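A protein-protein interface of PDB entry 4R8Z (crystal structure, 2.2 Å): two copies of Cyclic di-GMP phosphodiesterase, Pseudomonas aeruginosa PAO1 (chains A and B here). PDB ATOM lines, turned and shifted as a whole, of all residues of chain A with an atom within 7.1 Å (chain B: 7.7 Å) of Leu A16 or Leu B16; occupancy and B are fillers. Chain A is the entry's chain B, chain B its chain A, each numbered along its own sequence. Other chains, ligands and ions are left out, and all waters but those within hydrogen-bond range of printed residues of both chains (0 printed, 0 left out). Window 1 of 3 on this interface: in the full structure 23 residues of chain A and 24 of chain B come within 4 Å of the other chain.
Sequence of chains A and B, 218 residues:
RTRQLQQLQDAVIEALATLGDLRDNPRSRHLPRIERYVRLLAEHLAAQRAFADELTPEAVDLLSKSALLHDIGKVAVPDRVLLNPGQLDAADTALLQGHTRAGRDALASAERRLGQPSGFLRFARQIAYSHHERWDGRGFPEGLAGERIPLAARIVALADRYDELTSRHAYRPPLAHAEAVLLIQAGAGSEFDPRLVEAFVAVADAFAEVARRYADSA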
ATOM      1  N   ASP A  10       7.555 -28.683  -0.078  1.00  0.00           N
ATOM      2  CA  ASP A  10       7.319 -27.737  -1.152  1.00  0.00           C
ATOM      3  C   ASP A  10       6.031 -28.043  -1.847  1.00  0.00           C
ATOM      4  O   ASP A  10       5.283 -27.154  -2.177  1.00  0.00           O
ATOM      5  CB  ASP A  10       8.442 -27.735  -2.183  1.00  0.00           C
ATOM      6  CG  ASP A  10       9.770 -27.234  -1.588  1.00  0.00           C
ATOM      7  OD1 ASP A  10       9.771 -26.824  -0.395  1.00  0.00           O
ATOM      8  OD2 ASP A  10      10.830 -27.286  -2.280  1.00  0.00           O
ATOM      9  N   ALA A  11       5.756 -29.310  -2.090  1.00  0.00           N
ATOM     10  CA  ALA A  11       4.507 -29.656  -2.790  1.00  0.00           C
ATOM     11  C   ALA A  11       3.249 -29.310  -1.988  1.00  0.00           C
ATOM     12  O   ALA A  11       2.290 -28.750  -2.522  1.00  0.00           O
ATOM     13  CB  ALA A  11       4.520 -31.132  -3.141  1.00  0.00           C
ATOM     14  N   VAL A  12       3.295 -29.597  -0.695  1.00  0.00           N
ATOM     15  CA  VAL A  12       2.175 -29.337   0.153  1.00  0.00           C
ATOM     16  C   VAL A  12       1.951 -27.855   0.348  1.00  0.00           C
ATOM     17  O   VAL A  12       0.824 -27.374   0.350  1.00  0.00           O
ATOM     18  CB  VAL A  12       2.358 -29.941   1.555  1.00  0.00           C
ATOM     19  CG1 VAL A  12       1.068 -29.833   2.348  1.00  0.00           C
ATOM     20  CG2 VAL A  12       2.699 -31.413   1.470  1.00  0.00           C
ATOM     21  N   ILE A  13       3.002 -27.124   0.596  1.00  0.00           N
ATOM     22  CA  ILE A  13       2.839 -25.689   0.726  1.00  0.00           C
ATOM     23  C   ILE A  13       2.272 -25.037  -0.504  1.00  0.00           C
ATOM     24  O   ILE A  13       1.392 -24.189  -0.407  1.00  0.00           O
ATOM     25  CB  ILE A  13       4.130 -25.023   1.123  1.00  0.00           C
ATOM     26  CG1 ILE A  13       4.281 -25.243   2.615  1.00  0.00           C
ATOM     27  CG2 ILE A  13       4.084 -23.524   0.876  1.00  0.00           C
ATOM     28  CD1 ILE A  13       5.684 -24.963   3.013  1.00  0.00           C
ATOM     29  N   GLU A  14       2.742 -25.437  -1.662  1.00  0.00           N
ATOM     30  CA  GLU A  14       2.227 -24.865  -2.878  1.00  0.00           C
ATOM     31  C   GLU A  14       0.765 -25.221  -3.018  1.00  0.00           C
ATOM     32  O   GLU A  14      -0.037 -24.366  -3.348  1.00  0.00           O
ATOM     33  CB  GLU A  14       3.058 -25.290  -4.091  1.00  0.00           C
ATOM     34  CG  GLU A  14       2.587 -24.660  -5.389  1.00  0.00           C
ATOM     35  CD  GLU A  14       2.812 -25.526  -6.663  1.00  0.00           C
ATOM     36  OE1 GLU A  14       2.869 -26.818  -6.625  1.00  0.00           O
ATOM     37  OE2 GLU A  14       2.936 -24.855  -7.735  1.00  0.00           O
ATOM     38  N   ALA A  15       0.388 -26.472  -2.760  1.00  0.00           N
ATOM     39  CA  ALA A  15      -1.039 -26.840  -2.868  1.00  0.00           C
ATOM     40  C   ALA A  15      -1.930 -26.029  -1.932  1.00  0.00           C
ATOM     41  O   ALA A  15      -2.956 -25.570  -2.309  1.00  0.00           O
ATOM     42  CB  ALA A  15      -1.210 -28.300  -2.568  1.00  0.00           C
ATOM     43  N   LEU A  16      -1.500 -25.805  -0.719  1.00  0.00           N
ATOM     44  CA  LEU A  16      -2.348 -25.092   0.240  1.00  0.00           C
ATOM     45  C   LEU A  16      -2.374 -23.618  -0.006  1.00  0.00           C
ATOM     46  O   LEU A  16      -3.392 -22.963   0.156  1.00  0.00           O
ATOM     47  CB  LEU A  16      -1.810 -25.332   1.644  1.00  0.00           C
ATOM     48  CG  LEU A  16      -1.921 -26.812   2.056  1.00  0.00           C
ATOM     49  CD1 LEU A  16      -1.427 -26.986   3.459  1.00  0.00           C
ATOM     50  CD2 LEU A  16      -3.326 -27.346   1.933  1.00  0.00           C
ATOM     51  N   ALA A  17      -1.250 -23.071  -0.430  1.00  0.00           N
ATOM     52  CA  ALA A  17      -1.251 -21.663  -0.803  1.00  0.00           C
ATOM     53  C   ALA A  17      -2.185 -21.404  -1.972  1.00  0.00           C
ATOM     54  O   ALA A  17      -2.902 -20.400  -2.013  1.00  0.00           O
ATOM     55  CB  ALA A  17       0.149 -21.228  -1.151  1.00  0.00           C
ATOM     56  N   THR A  18      -2.194 -22.313  -2.911  1.00  0.00           N
ATOM     57  CA  THR A  18      -3.080 -22.244  -4.112  1.00  0.00           C
ATOM     58  C   THR A  18      -4.555 -22.347  -3.825  1.00  0.00           C
ATOM     59  O   THR A  18      -5.351 -21.519  -4.315  1.00  0.00           O
ATOM     60  CB  THR A  18      -2.667 -23.288  -5.129  1.00  0.00           C
ATOM     61  OG1 THR A  18      -1.302 -23.036  -5.468  1.00  0.00           O
ATOM     62  CG2 THR A  18      -3.469 -23.145  -6.397  1.00  0.00           C
ATOM     63  N   LEU A  19      -4.922 -23.277  -2.939  1.00  0.00           N
ATOM     64  CA  LEU A  19      -6.257 -23.281  -2.358  1.00  0.00           C
ATOM     65  C   LEU A  19      -6.595 -22.000  -1.624  1.00  0.00           C
ATOM     66  O   LEU A  19      -7.737 -21.558  -1.663  1.00  0.00           O
ATOM     67  CB  LEU A  19      -6.427 -24.469  -1.392  1.00  0.00           C
ATOM     68  CG  LEU A  19      -6.839 -25.805  -1.984  1.00  0.00           C
ATOM     69  CD1 LEU A  19      -7.000 -26.835  -0.862  1.00  0.00           C
ATOM     70  CD2 LEU A  19      -8.110 -25.765  -2.845  1.00  0.00           C
ATOM     71  N   GLY A  20      -5.637 -21.396  -0.965  1.00  0.00           N
ATOM     72  CA  GLY A  20      -5.892 -20.066  -0.384  1.00  0.00           C
ATOM     73  C   GLY A  20      -6.181 -18.910  -1.355  1.00  0.00           C
ATOM     74  O   GLY A  20      -6.616 -17.834  -0.946  1.00  0.00           O
ATOM     75  N   ASP A  21      -5.916 -19.114  -2.628  1.00  0.00           N
ATOM     76  CA  ASP A  21      -6.188 -18.082  -3.640  1.00  0.00           C
ATOM     77  C   ASP A  21      -7.466 -18.367  -4.374  1.00  0.00           C
ATOM     78  O   ASP A  21      -7.893 -17.589  -5.231  1.00  0.00           O
ATOM     79  CB  ASP A  21      -5.042 -18.042  -4.672  1.00  0.00           C
ATOM     80  CG  ASP A  21      -3.939 -16.939  -4.359  1.00  0.00           C
ATOM     81  OD1 ASP A  21      -3.975 -16.270  -3.294  1.00  0.00           O
ATOM     82  OD2 ASP A  21      -2.990 -16.776  -5.195  1.00  0.00           O
ATOM     83  N   LEU A  31       1.414 -17.291  -7.883  1.00  0.00           N
ATOM     84  CA  LEU A  31       2.323 -17.808  -6.862  1.00  0.00           C
ATOM     85  C   LEU A  31       3.689 -18.212  -7.377  1.00  0.00           C
ATOM     86  O   LEU A  31       4.713 -17.813  -6.825  1.00  0.00           O
ATOM     87  CB  LEU A  31       1.680 -18.936  -6.087  1.00  0.00           C
ATOM     88  CG  LEU A  31       0.430 -18.508  -5.316  1.00  0.00           C
ATOM     89  CD1 LEU A  31      -0.277 -19.668  -4.614  1.00  0.00           C
ATOM     90  CD2 LEU A  31       0.732 -17.386  -4.316  1.00  0.00           C
ATOM     91  N   LEU A  68       5.212 -17.567  -0.658  1.00  0.00           N
ATOM     92  CA  LEU A  68       3.954 -18.164  -1.150  1.00  0.00           C
ATOM     93  C   LEU A  68       2.741 -18.015  -0.221  1.00  0.00           C
ATOM     94  O   LEU A  68       1.585 -18.048  -0.683  1.00  0.00           O
ATOM     95  CB  LEU A  68       4.172 -19.652  -1.415  1.00  0.00           C
ATOM     96  CG  LEU A  68       5.097 -20.090  -2.534  1.00  0.00           C
ATOM     97  CD1 LEU A  68       5.215 -21.628  -2.585  1.00  0.00           C
ATOM     98  CD2 LEU A  68       4.575 -19.641  -3.878  1.00  0.00           C
ATOM     99  N   LEU A  69       2.998 -17.911   1.074  1.00  0.00           N
ATOM    100  CA  LEU A  69       1.931 -17.815   2.061  1.00  0.00           C
ATOM    101  C   LEU A  69       1.448 -16.430   2.365  1.00  0.00           C
ATOM    102  O   LEU A  69       0.594 -16.284   3.241  1.00  0.00           O
ATOM    103  CB  LEU A  69       2.411 -18.459   3.389  1.00  0.00           C
ATOM    104  CG  LEU A  69       2.738 -19.963   3.231  1.00  0.00           C
ATOM    105  CD1 LEU A  69       3.375 -20.545   4.474  1.00  0.00           C
ATOM    106  CD2 LEU A  69       1.469 -20.763   2.885  1.00  0.00           C
ATOM    107  N   ILE A  72      -2.400 -16.034   2.688  1.00  0.00           N
ATOM    108  CA  ILE A  72      -3.145 -17.197   3.201  1.00  0.00           C
ATOM    109  C   ILE A  72      -4.287 -16.782   4.123  1.00  0.00           C
ATOM    110  O   ILE A  72      -5.298 -17.458   4.217  1.00  0.00           O
ATOM    111  CB  ILE A  72      -2.142 -18.185   3.876  1.00  0.00           C
ATOM    112  CG1 ILE A  72      -2.742 -19.578   3.926  1.00  0.00           C
ATOM    113  CG2 ILE A  72      -1.662 -17.761   5.277  1.00  0.00           C
ATOM    114  CD1 ILE A  72      -2.958 -20.266   2.582  1.00  0.00           C
ATOM    115  N   GLY A 103      -3.285 -14.166   8.850  1.00  0.00           N
ATOM    116  CA  GLY A 103      -2.190 -15.001   8.403  1.00  0.00           C
ATOM    117  C   GLY A 103      -1.099 -15.037   9.452  1.00  0.00           C
ATOM    118  O   GLY A 103      -0.499 -16.113   9.717  1.00  0.00           O
ATOM    119  N   ALA A 106      -2.097 -17.479  12.417  1.00  0.00           N
ATOM    120  CA  ALA A 106      -1.927 -18.894  12.068  1.00  0.00           C
ATOM    121  C   ALA A 106      -0.471 -19.286  12.050  1.00  0.00           C
ATOM    122  O   ALA A 106      -0.106 -20.304  12.573  1.00  0.00           O
ATOM    123  CB  ALA A 106      -2.575 -19.157  10.766  1.00  0.00           C
ATOM    124  N   LEU A 107       0.407 -18.467  11.475  1.00  0.00           N
ATOM    125  CA  LEU A 107       1.816 -18.832  11.414  1.00  0.00           C
ATOM    126  C   LEU A 107       2.530 -18.685  12.743  1.00  0.00           C
ATOM    127  O   LEU A 107       3.474 -19.448  13.029  1.00  0.00           O
ATOM    128  CB  LEU A 107       2.551 -18.045  10.358  1.00  0.00           C
ATOM    129  CG  LEU A 107       1.944 -18.381   8.955  1.00  0.00           C
ATOM    130  CD1 LEU A 107       2.212 -17.284   7.937  1.00  0.00           C
ATOM    131  CD2 LEU A 107       2.476 -19.688   8.415  1.00  0.00           C
ATOM    132  N   ALA A 110       1.760 -21.811  14.630  1.00  0.00           N
ATOM    133  CA  ALA A 110       2.662 -22.839  14.228  1.00  0.00           C
ATOM    134  C   ALA A 110       4.089 -22.768  14.825  1.00  0.00           C
ATOM    135  O   ALA A 110       4.717 -23.826  15.085  1.00  0.00           O
ATOM    136  CB  ALA A 110       2.776 -22.843  12.729  1.00  0.00           C
ATOM    137  N   ARG A 113       3.776 -24.235  18.270  1.00  0.00           N
ATOM    138  CA  ARG A 113       3.695 -25.679  18.231  1.00  0.00           C
ATOM    139  C   ARG A 113       5.047 -26.304  18.076  1.00  0.00           C
ATOM    140  O   ARG A 113       5.304 -27.384  18.616  1.00  0.00           O
ATOM    141  CB  ARG A 113       2.865 -26.195  17.067  1.00  0.00           C
ATOM    142  CG  ARG A 113       1.362 -25.999  17.164  1.00  0.00           C
ATOM    143  CD  ARG A 113       0.673 -26.504  15.881  1.00  0.00           C
ATOM    144  NE  ARG A 113      -0.434 -25.662  15.403  1.00  0.00           N
ATOM    145  CZ  ARG A 113      -1.616 -25.565  16.005  1.00  0.00           C
ATOM    146  NH1 ARG A 113      -1.834 -26.227  17.137  1.00  0.00           N
ATOM    147  NH2 ARG A 113      -2.575 -24.791  15.491  1.00  0.00           N
ATOM    148  N   ASP B  10       4.790 -31.043  10.352  1.00  0.00           N
ATOM    149  CA  ASP B  10       3.597 -31.272  11.141  1.00  0.00           C
ATOM    150  C   ASP B  10       3.032 -29.958  11.605  1.00  0.00           C
ATOM    151  O   ASP B  10       1.837 -29.770  11.615  1.00  0.00           O
ATOM    152  CB  ASP B  10       3.885 -32.165  12.364  1.00  0.00           C
ATOM    153  CG  ASP B  10       4.254 -33.626  11.976  1.00  0.00           C
ATOM    154  OD1 ASP B  10       4.145 -33.994  10.763  1.00  0.00           O
ATOM    155  OD2 ASP B  10       4.667 -34.402  12.901  1.00  0.00           O
ATOM    156  N   ALA B  11       3.884 -29.058  12.059  1.00  0.00           N
ATOM    157  CA  ALA B  11       3.406 -27.778  12.539  1.00  0.00           C
ATOM    158  C   ALA B  11       2.750 -26.930  11.459  1.00  0.00           C
ATOM    159  O   ALA B  11       1.708 -26.361  11.678  1.00  0.00           O
ATOM    160  CB  ALA B  11       4.511 -26.998  13.218  1.00  0.00           C
ATOM    161  N   VAL B  12       3.366 -26.881  10.293  1.00  0.00           N
ATOM    162  CA  VAL B  12       2.822 -26.133   9.196  1.00  0.00           C
ATOM    163  C   VAL B  12       1.498 -26.688   8.724  1.00  0.00           C
ATOM    164  O   VAL B  12       0.574 -25.956   8.553  1.00  0.00           O
ATOM    165  CB  VAL B  12       3.780 -26.097   8.000  1.00  0.00           C
ATOM    166  CG1 VAL B  12       3.172 -25.284   6.885  1.00  0.00           C
ATOM    167  CG2 VAL B  12       5.099 -25.498   8.394  1.00  0.00           C
ATOM    168  N   ILE B  13       1.406 -27.996   8.573  1.00  0.00           N
ATOM    169  CA  ILE B  13       0.179 -28.598   8.127  1.00  0.00           C
ATOM    170  C   ILE B  13      -0.925 -28.341   9.130  1.00  0.00           C
ATOM    171  O   ILE B  13      -1.999 -27.999   8.746  1.00  0.00           O
ATOM    172  CB  ILE B  13       0.337 -30.101   7.860  1.00  0.00           C
ATOM    173  CG1 ILE B  13       1.123 -30.320   6.594  1.00  0.00           C
ATOM    174  CG2 ILE B  13      -0.999 -30.813   7.718  1.00  0.00           C
ATOM    175  CD1 ILE B  13       1.428 -31.759   6.336  1.00  0.00           C
ATOM    176  N   GLU B  14      -0.619 -28.480  10.407  1.00  0.00           N
ATOM    177  CA  GLU B  14      -1.588 -28.284  11.456  1.00  0.00           C
ATOM    178  C   GLU B  14      -2.081 -26.834  11.384  1.00  0.00           C
ATOM    179  O   GLU B  14      -3.254 -26.587  11.381  1.00  0.00           O
ATOM    180  CB  GLU B  14      -0.922 -28.502  12.819  1.00  0.00           C
ATOM    181  N   ALA B  15      -1.162 -25.895  11.236  1.00  0.00           N
ATOM    182  CA  ALA B  15      -1.544 -24.498  11.227  1.00  0.00           C
ATOM    183  C   ALA B  15      -2.464 -24.134  10.082  1.00  0.00           C
ATOM    184  O   ALA B  15      -3.448 -23.464  10.268  1.00  0.00           O
ATOM    185  CB  ALA B  15      -0.320 -23.622  11.208  1.00  0.00           C
ATOM    186  N   LEU B  16      -2.154 -24.631   8.907  1.00  0.00           N
ATOM    187  CA  LEU B  16      -2.888 -24.260   7.717  1.00  0.00           C
ATOM    188  C   LEU B  16      -4.212 -25.016   7.531  1.00  0.00           C
ATOM    189  O   LEU B  16      -5.177 -24.482   6.992  1.00  0.00           O
ATOM    190  CB  LEU B  16      -2.060 -24.588   6.480  1.00  0.00           C
ATOM    191  CG  LEU B  16      -0.756 -23.753   6.426  1.00  0.00           C
ATOM    192  CD1 LEU B  16      -0.053 -24.038   5.098  1.00  0.00           C
ATOM    193  CD2 LEU B  16      -0.975 -22.259   6.593  1.00  0.00           C
ATOM    194  N   ALA B  17      -4.244 -26.285   7.934  1.00  0.00           N
ATOM    195  CA  ALA B  17      -5.509 -26.955   8.002  1.00  0.00           C
ATOM    196  C   ALA B  17      -6.461 -26.184   8.927  1.00  0.00           C
ATOM    197  O   ALA B  17      -7.624 -26.126   8.681  1.00  0.00           O
ATOM    198  CB  ALA B  17      -5.296 -28.392   8.522  1.00  0.00           C
ATOM    199  N   THR B  18      -5.930 -25.672  10.029  1.00  0.00           N
ATOM    200  CA  THR B  18      -6.691 -24.891  11.000  1.00  0.00           C
ATOM    201  C   THR B  18      -7.249 -23.605  10.475  1.00  0.00           C
ATOM    202  O   THR B  18      -8.443 -23.332  10.662  1.00  0.00           O
ATOM    203  CB  THR B  18      -5.883 -24.644  12.275  1.00  0.00           C
ATOM    204  OG1 THR B  18      -5.515 -25.921  12.834  1.00  0.00           O
ATOM    205  CG2 THR B  18      -6.722 -23.953  13.327  1.00  0.00           C
ATOM    206  N   LEU B  19      -6.438 -22.850   9.735  1.00  0.00           N
ATOM    207  CA  LEU B  19      -6.962 -21.748   8.933  1.00  0.00           C
ATOM    208  C   LEU B  19      -8.042 -22.195   7.986  1.00  0.00           C
ATOM    209  O   LEU B  19      -9.015 -21.473   7.765  1.00  0.00           O
ATOM    210  CB  LEU B  19      -5.898 -21.121   8.026  1.00  0.00           C
ATOM    211  CG  LEU B  19      -5.276 -19.747   8.264  1.00  0.00           C
ATOM    212  CD1 LEU B  19      -4.479 -19.314   7.034  1.00  0.00           C
ATOM    213  CD2 LEU B  19      -6.256 -18.660   8.671  1.00  0.00           C
ATOM    214  N   GLY B  20      -7.831 -23.325   7.312  1.00  0.00           N
ATOM    215  CA  GLY B  20      -8.870 -23.779   6.413  1.00  0.00           C
ATOM    216  C   GLY B  20     -10.223 -24.076   7.087  1.00  0.00           C
ATOM    217  O   GLY B  20     -11.203 -24.360   6.387  1.00  0.00           O
ATOM    218  N   ASP B  21     -10.270 -24.131   8.413  1.00  0.00           N
ATOM    219  CA  ASP B  21     -11.524 -24.387   9.159  1.00  0.00           C
ATOM    220  C   ASP B  21     -12.114 -23.051   9.644  1.00  0.00           C
ATOM    221  O   ASP B  21     -13.163 -23.024  10.279  1.00  0.00           O
ATOM    222  CB  ASP B  21     -11.214 -25.246  10.394  1.00  0.00           C
ATOM    223  CG  ASP B  21     -11.495 -26.789  10.201  1.00  0.00           C
ATOM    224  OD1 ASP B  21     -11.860 -27.232   9.077  1.00  0.00           O
ATOM    225  OD2 ASP B  21     -11.357 -27.551  11.239  1.00  0.00           O
ATOM    226  N   LEU B  22     -11.386 -21.948   9.455  1.00  0.00           N
ATOM    227  CA  LEU B  22     -11.742 -20.706  10.095  1.00  0.00           C
ATOM    228  C   LEU B  22     -13.137 -20.248   9.665  1.00  0.00           C
ATOM    229  O   LEU B  22     -13.890 -19.696  10.457  1.00  0.00           O
ATOM    230  CB  LEU B  22     -10.750 -19.632   9.721  1.00  0.00           C
ATOM    231  CG  LEU B  22     -10.981 -18.316  10.439  1.00  0.00           C
ATOM    232  CD1 LEU B  22     -10.371 -18.385  11.841  1.00  0.00           C
ATOM    233  CD2 LEU B  22     -10.409 -17.151   9.682  1.00  0.00           C
ATOM    234  N   LEU B  31      -9.458 -30.824  14.733  1.00  0.00           N
ATOM    235  CA  LEU B  31      -8.386 -31.465  14.011  1.00  0.00           C
ATOM    236  C   LEU B  31      -7.506 -32.387  14.859  1.00  0.00           C
ATOM    237  O   LEU B  31      -7.239 -33.524  14.480  1.00  0.00           O
ATOM    238  CB  LEU B  31      -7.517 -30.450  13.282  1.00  0.00           C
ATOM    239  CG  LEU B  31      -8.311 -29.679  12.255  1.00  0.00           C
ATOM    240  CD1 LEU B  31      -7.517 -28.569  11.592  1.00  0.00           C
ATOM    241  CD2 LEU B  31      -8.944 -30.587  11.198  1.00  0.00           C
ATOM    242  N   LEU B  68      -5.907 -34.809   8.811  1.00  0.00           N
ATOM    243  CA  LEU B  68      -6.056 -33.382   9.068  1.00  0.00           C
ATOM    244  C   LEU B  68      -6.521 -32.538   7.860  1.00  0.00           C
ATOM    245  O   LEU B  68      -7.109 -31.440   8.034  1.00  0.00           O
ATOM    246  CB  LEU B  68      -4.727 -32.785   9.532  1.00  0.00           C
ATOM    247  CG  LEU B  68      -4.163 -33.204  10.872  1.00  0.00           C
ATOM    248  CD1 LEU B  68      -2.827 -32.502  11.138  1.00  0.00           C
ATOM    249  CD2 LEU B  68      -5.070 -32.835  11.984  1.00  0.00           C
ATOM    250  N   LEU B  69      -6.213 -33.009   6.666  1.00  0.00           N
ATOM    251  CA  LEU B  69      -6.535 -32.247   5.457  1.00  0.00           C
ATOM    252  C   LEU B  69      -7.918 -32.558   4.852  1.00  0.00           C
ATOM    253  O   LEU B  69      -8.207 -32.092   3.731  1.00  0.00           O
ATOM    254  CB  LEU B  69      -5.445 -32.507   4.409  1.00  0.00           C
ATOM    255  CG  LEU B  69      -4.082 -31.993   4.839  1.00  0.00           C
ATOM    256  CD1 LEU B  69      -2.960 -32.432   3.921  1.00  0.00           C
ATOM    257  CD2 LEU B  69      -4.084 -30.446   4.905  1.00  0.00           C
ATOM    258  N   ILE B  72      -9.965 -29.421   3.613  1.00  0.00           N
ATOM    259  CA  ILE B  72      -9.291 -28.173   3.108  1.00  0.00           C
ATOM    260  C   ILE B  72      -9.924 -27.590   1.846  1.00  0.00           C
ATOM    261  O   ILE B  72      -9.774 -26.424   1.558  1.00  0.00           O
ATOM    262  CB  ILE B  72      -7.840 -28.443   2.649  1.00  0.00           C
ATOM    263  CG1 ILE B  72      -7.851 -29.593   1.669  1.00  0.00           C
ATOM    264  CG2 ILE B  72      -6.952 -28.632   3.827  1.00  0.00           C
ATOM    265  CD1 ILE B  72      -6.495 -30.026   1.214  1.00  0.00           C
ATOM    266  N   GLY B  73     -10.656 -28.424   1.109  1.00  0.00           N
ATOM    267  CA  GLY B  73     -11.424 -27.990  -0.014  1.00  0.00           C
ATOM    268  C   GLY B  73     -12.612 -27.075   0.215  1.00  0.00           C
ATOM    269  O   GLY B  73     -13.243 -26.599  -0.749  1.00  0.00           O
ATOM    270  N   VAL B  75     -12.761 -24.026   0.934  1.00  0.00           N
ATOM    271  CA  VAL B  75     -12.618 -22.746   0.242  1.00  0.00           C
ATOM    272  C   VAL B  75     -13.363 -22.710  -1.082  1.00  0.00           C
ATOM    273  O   VAL B  75     -13.690 -21.636  -1.530  1.00  0.00           O
ATOM    274  CB  VAL B  75     -11.161 -22.332  -0.055  1.00  0.00           C
ATOM    275  CG1 VAL B  75     -10.452 -21.935   1.199  1.00  0.00           C
ATOM    276  CG2 VAL B  75     -10.420 -23.440  -0.785  1.00  0.00           C
ATOM    277  N   GLY B 103     -10.461 -30.540  -2.757  1.00  0.00           N
ATOM    278  CA  GLY B 103      -9.357 -30.951  -1.911  1.00  0.00           C
ATOM    279  C   GLY B 103      -8.575 -31.983  -2.696  1.00  0.00           C
ATOM    280  O   GLY B 103      -7.348 -31.979  -2.673  1.00  0.00           O
ATOM    281  N   ALA B 106      -6.269 -30.411  -5.479  1.00  0.00           N
ATOM    282  CA  ALA B 106      -5.097 -29.759  -4.978  1.00  0.00           C
ATOM    283  C   ALA B 106      -4.052 -30.774  -4.525  1.00  0.00           C
ATOM    284  O   ALA B 106      -2.874 -30.604  -4.796  1.00  0.00           O
ATOM    285  CB  ALA B 106      -5.483 -28.868  -3.830  1.00  0.00           C
ATOM    286  N   LEU B 107      -4.479 -31.842  -3.861  1.00  0.00           N
ATOM    287  CA  LEU B 107      -3.549 -32.792  -3.376  1.00  0.00           C
ATOM    288  C   LEU B 107      -3.020 -33.678  -4.491  1.00  0.00           C
ATOM    289  O   LEU B 107      -1.901 -34.169  -4.391  1.00  0.00           O
ATOM    290  CB  LEU B 107      -4.155 -33.677  -2.234  1.00  0.00           C
ATOM    291  CG  LEU B 107      -4.489 -32.827  -1.001  1.00  0.00           C
ATOM    292  CD1 LEU B 107      -5.509 -33.511  -0.120  1.00  0.00           C
ATOM    293  CD2 LEU B 107      -3.256 -32.558  -0.195  1.00  0.00           C
ATOM    294  N   ALA B 110      -0.271 -31.839  -6.066  1.00  0.00           N
ATOM    295  CA  ALA B 110       0.936 -31.943  -5.257  1.00  0.00           C
ATOM    296  C   ALA B 110       1.648 -33.295  -5.424  1.00  0.00           C
ATOM    297  O   ALA B 110       2.885 -33.353  -5.423  1.00  0.00           O
ATOM    298  CB  ALA B 110       0.644 -31.696  -3.786  1.00  0.00           C
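Ala B110 touches Ala A11 (O to CB, 3.6 Å).
Ala B106 touches Ala A15.
Leu B16 touches Leu A16 (CD1 to CD1, 3.6 Å).
CG2 of Val B75 touches O of Leu A19, at 3.4 Å.
Ala B106 touches Leu A19 (CB to CG, 3.8 Å).
O of Ile A72 touches CD1 of Leu B19, at 3.5 Å.
Ala A106 touches Leu B19 (CB to CG, 3.7 Å).
Ala A110 touches Ala B11.
CB of Ala A110 touches CB of Ala B15, at 3.5 Å.
Arg A113 touches Glu B14 (NE to CB, 3.9 Å).
O of Glu B14 sits at hydrogen-bond distance from OG1 of Thr B18 (2.8 Å).
Of the 23 printed residues of chain B, 9 touch a printed residue of chain A.
Printed residues of chain B that touch a printed residue of chain A: Ala B11, Glu B14, Ala B15, Leu B16, Leu B19, Ile B72, Val B75, Ala B106 and Ala B110.
Hydrophobic or aromatic side chains of chain B within 4 Å of the printed part of chain A: Ala B11, Ala B15, Leu B16, Leu B19, Ile B72, Val B75, Ala B106 and Ala B110.
Hydrophobic or aromatic side chains of chain A that line the printed part of chain B: Ala A11, Ala A15, Leu A16, Leu A19, Ile A72, Ala A106 and Ala A110.
Among the printed residues, 12 pairs touch across the chains.
Ala A15 touches Ala B106, and with the chains exchanged Ala A106 touches Ala B15.
Leu A16 touches its own counterpart, Leu B16.
Leu A19 touches Ala B106, and with the chains exchanged Ala A106 touches Leu B19.
Ala A110 touches Ala B15, but with the chains exchanged Ala A15 does not touch Ala B110 (4.1 Å).
20 positions are printed for both chains.
Leu A16 touches just one residue of chain B: Leu B16.
Leu B16 touches just one residue of chain A: Leu A16 (3.6 Å).
Printed residues of chain A within 4 Å of Ile B72: Leu A19.
Printed residues of chain A within 4 Å of Ala B15: Ala A106 and Ala A110.
Of the printed residues of chain B, Ala A11 touches Ala B110 (3.6 Å).
Of the printed residues of chain B, Ala A106 touches Ala B15 (3.6 Å) and Leu B19 (3.7 Å).
Printed residues of chain B within 4 Å of Leu A19: Ile B72, Val B75 and Ala B106.
The nearest printed residue of chain A that does not touch Glu B14 is Ala A110 (6.4 Å).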
